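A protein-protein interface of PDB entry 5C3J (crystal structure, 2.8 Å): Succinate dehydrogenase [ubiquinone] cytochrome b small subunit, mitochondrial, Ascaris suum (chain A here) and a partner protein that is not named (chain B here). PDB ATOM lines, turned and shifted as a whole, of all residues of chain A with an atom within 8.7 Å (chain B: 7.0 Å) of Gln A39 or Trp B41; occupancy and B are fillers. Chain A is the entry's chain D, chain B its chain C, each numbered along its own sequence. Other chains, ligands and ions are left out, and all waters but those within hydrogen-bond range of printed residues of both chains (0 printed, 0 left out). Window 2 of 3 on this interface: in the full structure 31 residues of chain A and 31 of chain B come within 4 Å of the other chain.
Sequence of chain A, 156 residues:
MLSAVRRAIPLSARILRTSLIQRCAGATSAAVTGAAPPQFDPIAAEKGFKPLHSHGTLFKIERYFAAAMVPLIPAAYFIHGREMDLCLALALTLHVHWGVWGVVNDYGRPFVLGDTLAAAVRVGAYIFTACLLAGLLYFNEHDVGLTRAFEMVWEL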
ATOM      1  N   ALA A  36     -12.081   9.218   7.686  1.00  0.00           N
ATOM      2  CA  ALA A  36     -11.261   8.865   8.835  1.00  0.00           C
ATOM      3  C   ALA A  36      -9.951   9.607   8.721  1.00  0.00           C
ATOM      4  O   ALA A  36      -9.439   9.751   7.613  1.00  0.00           O
ATOM      5  CB  ALA A  36     -10.996   7.368   8.865  1.00  0.00           C
ATOM      6  N   PRO A  37      -9.408  10.090   9.854  1.00  0.00           N
ATOM      7  CA  PRO A  37      -8.115  10.754   9.790  1.00  0.00           C
ATOM      8  C   PRO A  37      -7.005   9.754   9.448  1.00  0.00           C
ATOM      9  O   PRO A  37      -7.228   8.539   9.529  1.00  0.00           O
ATOM     10  CB  PRO A  37      -7.949  11.322  11.196  1.00  0.00           C
ATOM     11  CG  PRO A  37      -8.725  10.395  12.050  1.00  0.00           C
ATOM     12  CD  PRO A  37      -9.911  10.002  11.232  1.00  0.00           C
ATOM     13  N   PRO A  38      -5.823  10.253   9.055  1.00  0.00           N
ATOM     14  CA  PRO A  38      -4.764   9.341   8.661  1.00  0.00           C
ATOM     15  C   PRO A  38      -4.221   8.608   9.878  1.00  0.00           C
ATOM     16  O   PRO A  38      -3.828   9.241  10.862  1.00  0.00           O
ATOM     17  CB  PRO A  38      -3.702  10.255   8.045  1.00  0.00           C
ATOM     18  CG  PRO A  38      -4.173  11.654   8.251  1.00  0.00           C
ATOM     19  CD  PRO A  38      -5.329  11.626   9.196  1.00  0.00           C
ATOM     20  N   GLN A  39      -4.228   7.282   9.805  1.00  0.00           N
ATOM     21  CA  GLN A  39      -3.903   6.433  10.943  1.00  0.00           C
ATOM     22  C   GLN A  39      -3.260   5.160  10.407  1.00  0.00           C
ATOM     23  O   GLN A  39      -3.781   4.549   9.475  1.00  0.00           O
ATOM     24  CB  GLN A  39      -5.179   6.117  11.743  1.00  0.00           C
ATOM     25  CG  GLN A  39      -5.064   4.962  12.733  1.00  0.00           C
ATOM     26  CD  GLN A  39      -6.331   4.767  13.557  1.00  0.00           C
ATOM     27  OE1 GLN A  39      -7.061   5.728  13.844  1.00  0.00           O
ATOM     28  NE2 GLN A  39      -6.602   3.518  13.944  1.00  0.00           N
ATOM     29  N   PHE A  40      -2.125   4.778  10.979  1.00  0.00           N
ATOM     30  CA  PHE A  40      -1.403   3.588  10.546  1.00  0.00           C
ATOM     31  C   PHE A  40      -2.030   2.364  11.179  1.00  0.00           C
ATOM     32  O   PHE A  40      -1.862   2.136  12.373  1.00  0.00           O
ATOM     33  CB  PHE A  40       0.063   3.688  10.960  1.00  0.00           C
ATOM     34  CG  PHE A  40       0.894   2.508  10.553  1.00  0.00           C
ATOM     35  CD1 PHE A  40       1.444   2.440   9.276  1.00  0.00           C
ATOM     36  CD2 PHE A  40       1.156   1.487  11.438  1.00  0.00           C
ATOM     37  CE1 PHE A  40       2.224   1.365   8.889  1.00  0.00           C
ATOM     38  CE2 PHE A  40       1.934   0.408  11.055  1.00  0.00           C
ATOM     39  CZ  PHE A  40       2.468   0.348   9.778  1.00  0.00           C
ATOM     40  N   ASP A  41      -2.769   1.590  10.391  1.00  0.00           N
ATOM     41  CA  ASP A  41      -3.331   0.337  10.886  1.00  0.00           C
ATOM     42  C   ASP A  41      -2.289  -0.760  10.716  1.00  0.00           C
ATOM     43  O   ASP A  41      -2.014  -1.174   9.594  1.00  0.00           O
ATOM     44  CB  ASP A  41      -4.611  -0.032  10.155  1.00  0.00           C
ATOM     45  CG  ASP A  41      -5.248  -1.272  10.723  1.00  0.00           C
ATOM     46  OD1 ASP A  41      -5.898  -1.176  11.787  1.00  0.00           O
ATOM     47  OD2 ASP A  41      -5.088  -2.348  10.112  1.00  0.00           O
ATOM     48  N   PRO A  42      -1.706  -1.235  11.826  1.00  0.00           N
ATOM     49  CA  PRO A  42      -0.519  -2.067  11.735  1.00  0.00           C
ATOM     50  C   PRO A  42      -0.844  -3.540  11.512  1.00  0.00           C
ATOM     51  O   PRO A  42       0.076  -4.365  11.438  1.00  0.00           O
ATOM     52  CB  PRO A  42       0.119  -1.875  13.106  1.00  0.00           C
ATOM     53  CG  PRO A  42      -1.052  -1.735  14.020  1.00  0.00           C
ATOM     54  CD  PRO A  42      -2.158  -1.101  13.220  1.00  0.00           C
ATOM     55  N   ALA A  44      -3.360  -4.206   9.021  1.00  0.00           N
ATOM     56  CA  ALA A  44      -3.375  -4.051   7.572  1.00  0.00           C
ATOM     57  C   ALA A  44      -1.949  -4.212   7.028  1.00  0.00           C
ATOM     58  O   ALA A  44      -1.678  -5.078   6.190  1.00  0.00           O
ATOM     59  CB  ALA A  44      -3.946  -2.694   7.182  1.00  0.00           C
ATOM     60  N   ALA A  45      -1.037  -3.394   7.540  1.00  0.00           N
ATOM     61  CA  ALA A  45       0.355  -3.420   7.111  1.00  0.00           C
ATOM     62  C   ALA A  45       0.953  -4.837   7.074  1.00  0.00           C
ATOM     63  O   ALA A  45       1.778  -5.136   6.207  1.00  0.00           O
ATOM     64  CB  ALA A  45       1.185  -2.508   8.003  1.00  0.00           C
ATOM     65  N   THR B  36       9.368  -0.477   4.409  1.00  0.00           N
ATOM     66  CA  THR B  36       8.306  -1.071   5.248  1.00  0.00           C
ATOM     67  C   THR B  36       7.019  -0.291   5.090  1.00  0.00           C
ATOM     68  O   THR B  36       7.040   0.838   4.591  1.00  0.00           O
ATOM     69  CB  THR B  36       8.632  -0.957   6.738  1.00  0.00           C
ATOM     70  OG1 THR B  36       8.809   0.429   7.063  1.00  0.00           O
ATOM     71  CG2 THR B  36       9.885  -1.724   7.085  1.00  0.00           C
ATOM     72  N   PRO B  37       5.890  -0.863   5.548  1.00  0.00           N
ATOM     73  CA  PRO B  37       4.646  -0.085   5.515  1.00  0.00           C
ATOM     74  C   PRO B  37       4.723   1.224   6.318  1.00  0.00           C
ATOM     75  O   PRO B  37       4.230   2.251   5.840  1.00  0.00           O
ATOM     76  CB  PRO B  37       3.618  -1.047   6.108  1.00  0.00           C
ATOM     77  CG  PRO B  37       4.172  -2.400   5.819  1.00  0.00           C
ATOM     78  CD  PRO B  37       5.653  -2.238   6.025  1.00  0.00           C
ATOM     79  N   ILE B  38       5.358   1.188   7.497  1.00  0.00           N
ATOM     80  CA  ILE B  38       5.507   2.390   8.342  1.00  0.00           C
ATOM     81  C   ILE B  38       6.400   3.465   7.721  1.00  0.00           C
ATOM     82  O   ILE B  38       6.203   4.663   7.959  1.00  0.00           O
ATOM     83  CB  ILE B  38       5.994   2.062   9.791  1.00  0.00           C
ATOM     84  CG1 ILE B  38       5.972   3.315  10.688  1.00  0.00           C
ATOM     85  CG2 ILE B  38       7.393   1.460   9.806  1.00  0.00           C
ATOM     86  CD1 ILE B  38       4.619   4.004  10.791  1.00  0.00           C
ATOM     87  N   GLN B  39       7.378   3.043   6.928  1.00  0.00           N
ATOM     88  CA  GLN B  39       8.225   3.998   6.234  1.00  0.00           C
ATOM     89  C   GLN B  39       7.486   4.690   5.070  1.00  0.00           C
ATOM     90  O   GLN B  39       7.699   5.887   4.794  1.00  0.00           O
ATOM     91  CB  GLN B  39       9.482   3.301   5.777  1.00  0.00           C
ATOM     92  CG  GLN B  39      10.412   2.979   6.935  1.00  0.00           C
ATOM     93  CD  GLN B  39      11.626   2.148   6.533  1.00  0.00           C
ATOM     94  OE1 GLN B  39      11.509   1.090   5.901  1.00  0.00           O
ATOM     95  NE2 GLN B  39      12.799   2.615   6.927  1.00  0.00           N
ATOM     96  N   VAL B  40       6.596   3.946   4.415  1.00  0.00           N
ATOM     97  CA  VAL B  40       5.753   4.521   3.372  1.00  0.00           C
ATOM     98  C   VAL B  40       4.844   5.575   4.016  1.00  0.00           C
ATOM     99  O   VAL B  40       4.763   6.716   3.548  1.00  0.00           O
ATOM    100  CB  VAL B  40       4.916   3.443   2.625  1.00  0.00           C
ATOM    101  CG1 VAL B  40       3.959   4.093   1.634  1.00  0.00           C
ATOM    102  CG2 VAL B  40       5.822   2.468   1.893  1.00  0.00           C
ATOM    103  N   TRP B  41       4.183   5.184   5.104  1.00  0.00           N
ATOM    104  CA  TRP B  41       3.311   6.083   5.852  1.00  0.00           C
ATOM    105  C   TRP B  41       4.090   7.294   6.349  1.00  0.00           C
ATOM    106  O   TRP B  41       3.608   8.437   6.267  1.00  0.00           O
ATOM    107  CB  TRP B  41       2.694   5.356   7.054  1.00  0.00           C
ATOM    108  CG  TRP B  41       1.561   6.106   7.683  1.00  0.00           C
ATOM    109  CD1 TRP B  41       0.241   5.877   7.493  1.00  0.00           C
ATOM    110  CD2 TRP B  41       1.653   7.206   8.608  1.00  0.00           C
ATOM    111  NE1 TRP B  41      -0.505   6.759   8.233  1.00  0.00           N
ATOM    112  CE2 TRP B  41       0.336   7.588   8.928  1.00  0.00           C
ATOM    113  CE3 TRP B  41       2.722   7.900   9.203  1.00  0.00           C
ATOM    114  CZ2 TRP B  41       0.048   8.641   9.815  1.00  0.00           C
ATOM    115  CZ3 TRP B  41       2.434   8.952  10.084  1.00  0.00           C
ATOM    116  CH2 TRP B  41       1.106   9.309  10.375  1.00  0.00           C
ATOM    117  N   GLY B  42       5.282   7.029   6.882  1.00  0.00           N
ATOM    118  CA  GLY B  42       6.173   8.081   7.335  1.00  0.00           C
ATOM    119  C   GLY B  42       6.474   9.105   6.258  1.00  0.00           C
ATOM    120  O   GLY B  42       6.502  10.309   6.549  1.00  0.00           O
ATOM    121  N   TRP B  43       6.694   8.630   5.022  1.00  0.00           N
ATOM    122  CA  TRP B  43       6.995   9.525   3.910  1.00  0.00           C
ATOM    123  C   TRP B  43       5.771  10.377   3.557  1.00  0.00           C
ATOM    124  O   TRP B  43       5.897  11.595   3.356  1.00  0.00           O
ATOM    125  CB  TRP B  43       7.537   8.781   2.663  1.00  0.00           C
ATOM    126  CG  TRP B  43       7.743   9.736   1.508  1.00  0.00           C
ATOM    127  CD1 TRP B  43       6.923   9.910   0.424  1.00  0.00           C
ATOM    128  CD2 TRP B  43       8.781  10.717   1.387  1.00  0.00           C
ATOM    129  NE1 TRP B  43       7.397  10.937  -0.371  1.00  0.00           N
ATOM    130  CE2 TRP B  43       8.534  11.448   0.198  1.00  0.00           C
ATOM    131  CE3 TRP B  43       9.897  11.050   2.165  1.00  0.00           C
ATOM    132  CZ2 TRP B  43       9.375  12.480  -0.236  1.00  0.00           C
ATOM    133  CZ3 TRP B  43      10.726  12.091   1.739  1.00  0.00           C
ATOM    134  CH2 TRP B  43      10.461  12.789   0.548  1.00  0.00           C
ATOM    135  N   ASP B  44       4.590   9.766   3.494  1.00  0.00           N
ATOM    136  CA  ASP B  44       3.359  10.538   3.225  1.00  0.00           C
ATOM    137  C   ASP B  44       3.080  11.577   4.313  1.00  0.00           C
ATOM    138  O   ASP B  44       2.489  12.624   4.033  1.00  0.00           O
ATOM    139  CB  ASP B  44       2.144   9.619   3.061  1.00  0.00           C
ATOM    140  CG  ASP B  44       2.181   8.835   1.768  1.00  0.00           C
ATOM    141  OD1 ASP B  44       1.742   7.665   1.767  1.00  0.00           O
ATOM    142  OD2 ASP B  44       2.657   9.387   0.753  1.00  0.00           O
ATOM    143  N   TYR B  45       3.504  11.287   5.544  1.00  0.00           N
ATOM    144  CA  TYR B  45       3.408  12.253   6.628  1.00  0.00           C
ATOM    145  C   TYR B  45       4.198  13.523   6.305  1.00  0.00           C
ATOM    146  O   TYR B  45       3.681  14.651   6.415  1.00  0.00           O
ATOM    147  CB  TYR B  45       3.925  11.656   7.932  1.00  0.00           C
ATOM    148  CG  TYR B  45       3.922  12.638   9.082  1.00  0.00           C
ATOM    149  CD1 TYR B  45       2.732  13.067   9.661  1.00  0.00           C
ATOM    150  CD2 TYR B  45       5.109  13.144   9.583  1.00  0.00           C
ATOM    151  CE1 TYR B  45       2.735  13.967  10.713  1.00  0.00           C
ATOM    152  CE2 TYR B  45       5.122  14.041  10.634  1.00  0.00           C
ATOM    153  CZ  TYR B  45       3.934  14.449  11.197  1.00  0.00           C
ATOM    154  OH  TYR B  45       3.970  15.348  12.240  1.00  0.00           O
ATOM    155  N   LEU B  46       5.451  13.339   5.902  1.00  0.00           N
ATOM    156  CA  LEU B  46       6.307  14.474   5.605  1.00  0.00           C
ATOM    157  C   LEU B  46       5.686  15.373   4.530  1.00  0.00           C
ATOM    158  O   LEU B  46       5.657  16.606   4.688  1.00  0.00           O
ATOM    159  CB  LEU B  46       7.710  14.000   5.217  1.00  0.00           C
ATOM    160  CG  LEU B  46       8.503  13.369   6.377  1.00  0.00           C
ATOM    161  CD1 LEU B  46       9.809  12.738   5.914  1.00  0.00           C
ATOM    162  CD2 LEU B  46       8.778  14.402   7.453  1.00  0.00           C
ATOM    163  N   ARG B  48       2.412  15.549   3.581  1.00  0.00           N
ATOM    164  CA  ARG B  48       1.294  16.147   4.312  1.00  0.00           C
ATOM    165  C   ARG B  48       1.708  17.365   5.137  1.00  0.00           C
ATOM    166  O   ARG B  48       1.001  18.361   5.133  1.00  0.00           O
ATOM    167  CB  ARG B  48       0.629  15.127   5.225  1.00  0.00           C
ATOM    168  CG  ARG B  48      -0.769  14.725   4.821  1.00  0.00           C
ATOM    169  CD  ARG B  48      -1.333  13.765   5.855  1.00  0.00           C
ATOM    170  NE  ARG B  48      -0.818  12.414   5.634  1.00  0.00           N
ATOM    171  CZ  ARG B  48      -0.439  11.559   6.584  1.00  0.00           C
ATOM    172  NH1 ARG B  48      -0.476  11.887   7.880  1.00  0.00           N
ATOM    173  NH2 ARG B  48       0.011  10.356   6.227  1.00  0.00           N
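Ala A36 touches none of the printed residues of chain B.
Printed residues of chain B within 4 Å of Gln A39: Trp B41.
Of the printed residues of chain B, Phe A40 touches Pro B37 (3.6 Å), Ile B38 (3.4 Å) and Trp B41 (3.8 Å).
Of the printed residues of chain A, Pro B37 touches Phe A40 and Ala A45.
Of the printed residues of chain A, Ile B38 touches Phe A40.
No residue of chain A comes within 4 Å of Val B40.
Trp B41 touches just these residues of chain A: Gln A39 and Phe A40.
Printed residues of chain A within 4 Å of Arg B48: Pro A38.
The nearest residue of chain A that does not touch Trp B41 is Pro A38 (4.1 Å).
CB of Pro A38 touches NH1 of Arg B48, at 3.6 Å.
Gln A39 touches Trp B41.
Pro B37 touches Phe A40 (C to CE1, 3.6 Å).
Ile B38 touches Phe A40.
Trp B41 touches Phe A40.
Ala A45 touches Pro B37.
Hydrophobic or aromatic side chains of chain A that line the printed part of chain B: Pro A38, Phe A40 and Ala A45.
Of the 12 printed residues of chain B, 4 touch a printed residue of chain A.
Hydrophobic or aromatic side chains of chain B that line the printed part of chain A: Pro B37, Ile B38 and Trp B41.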
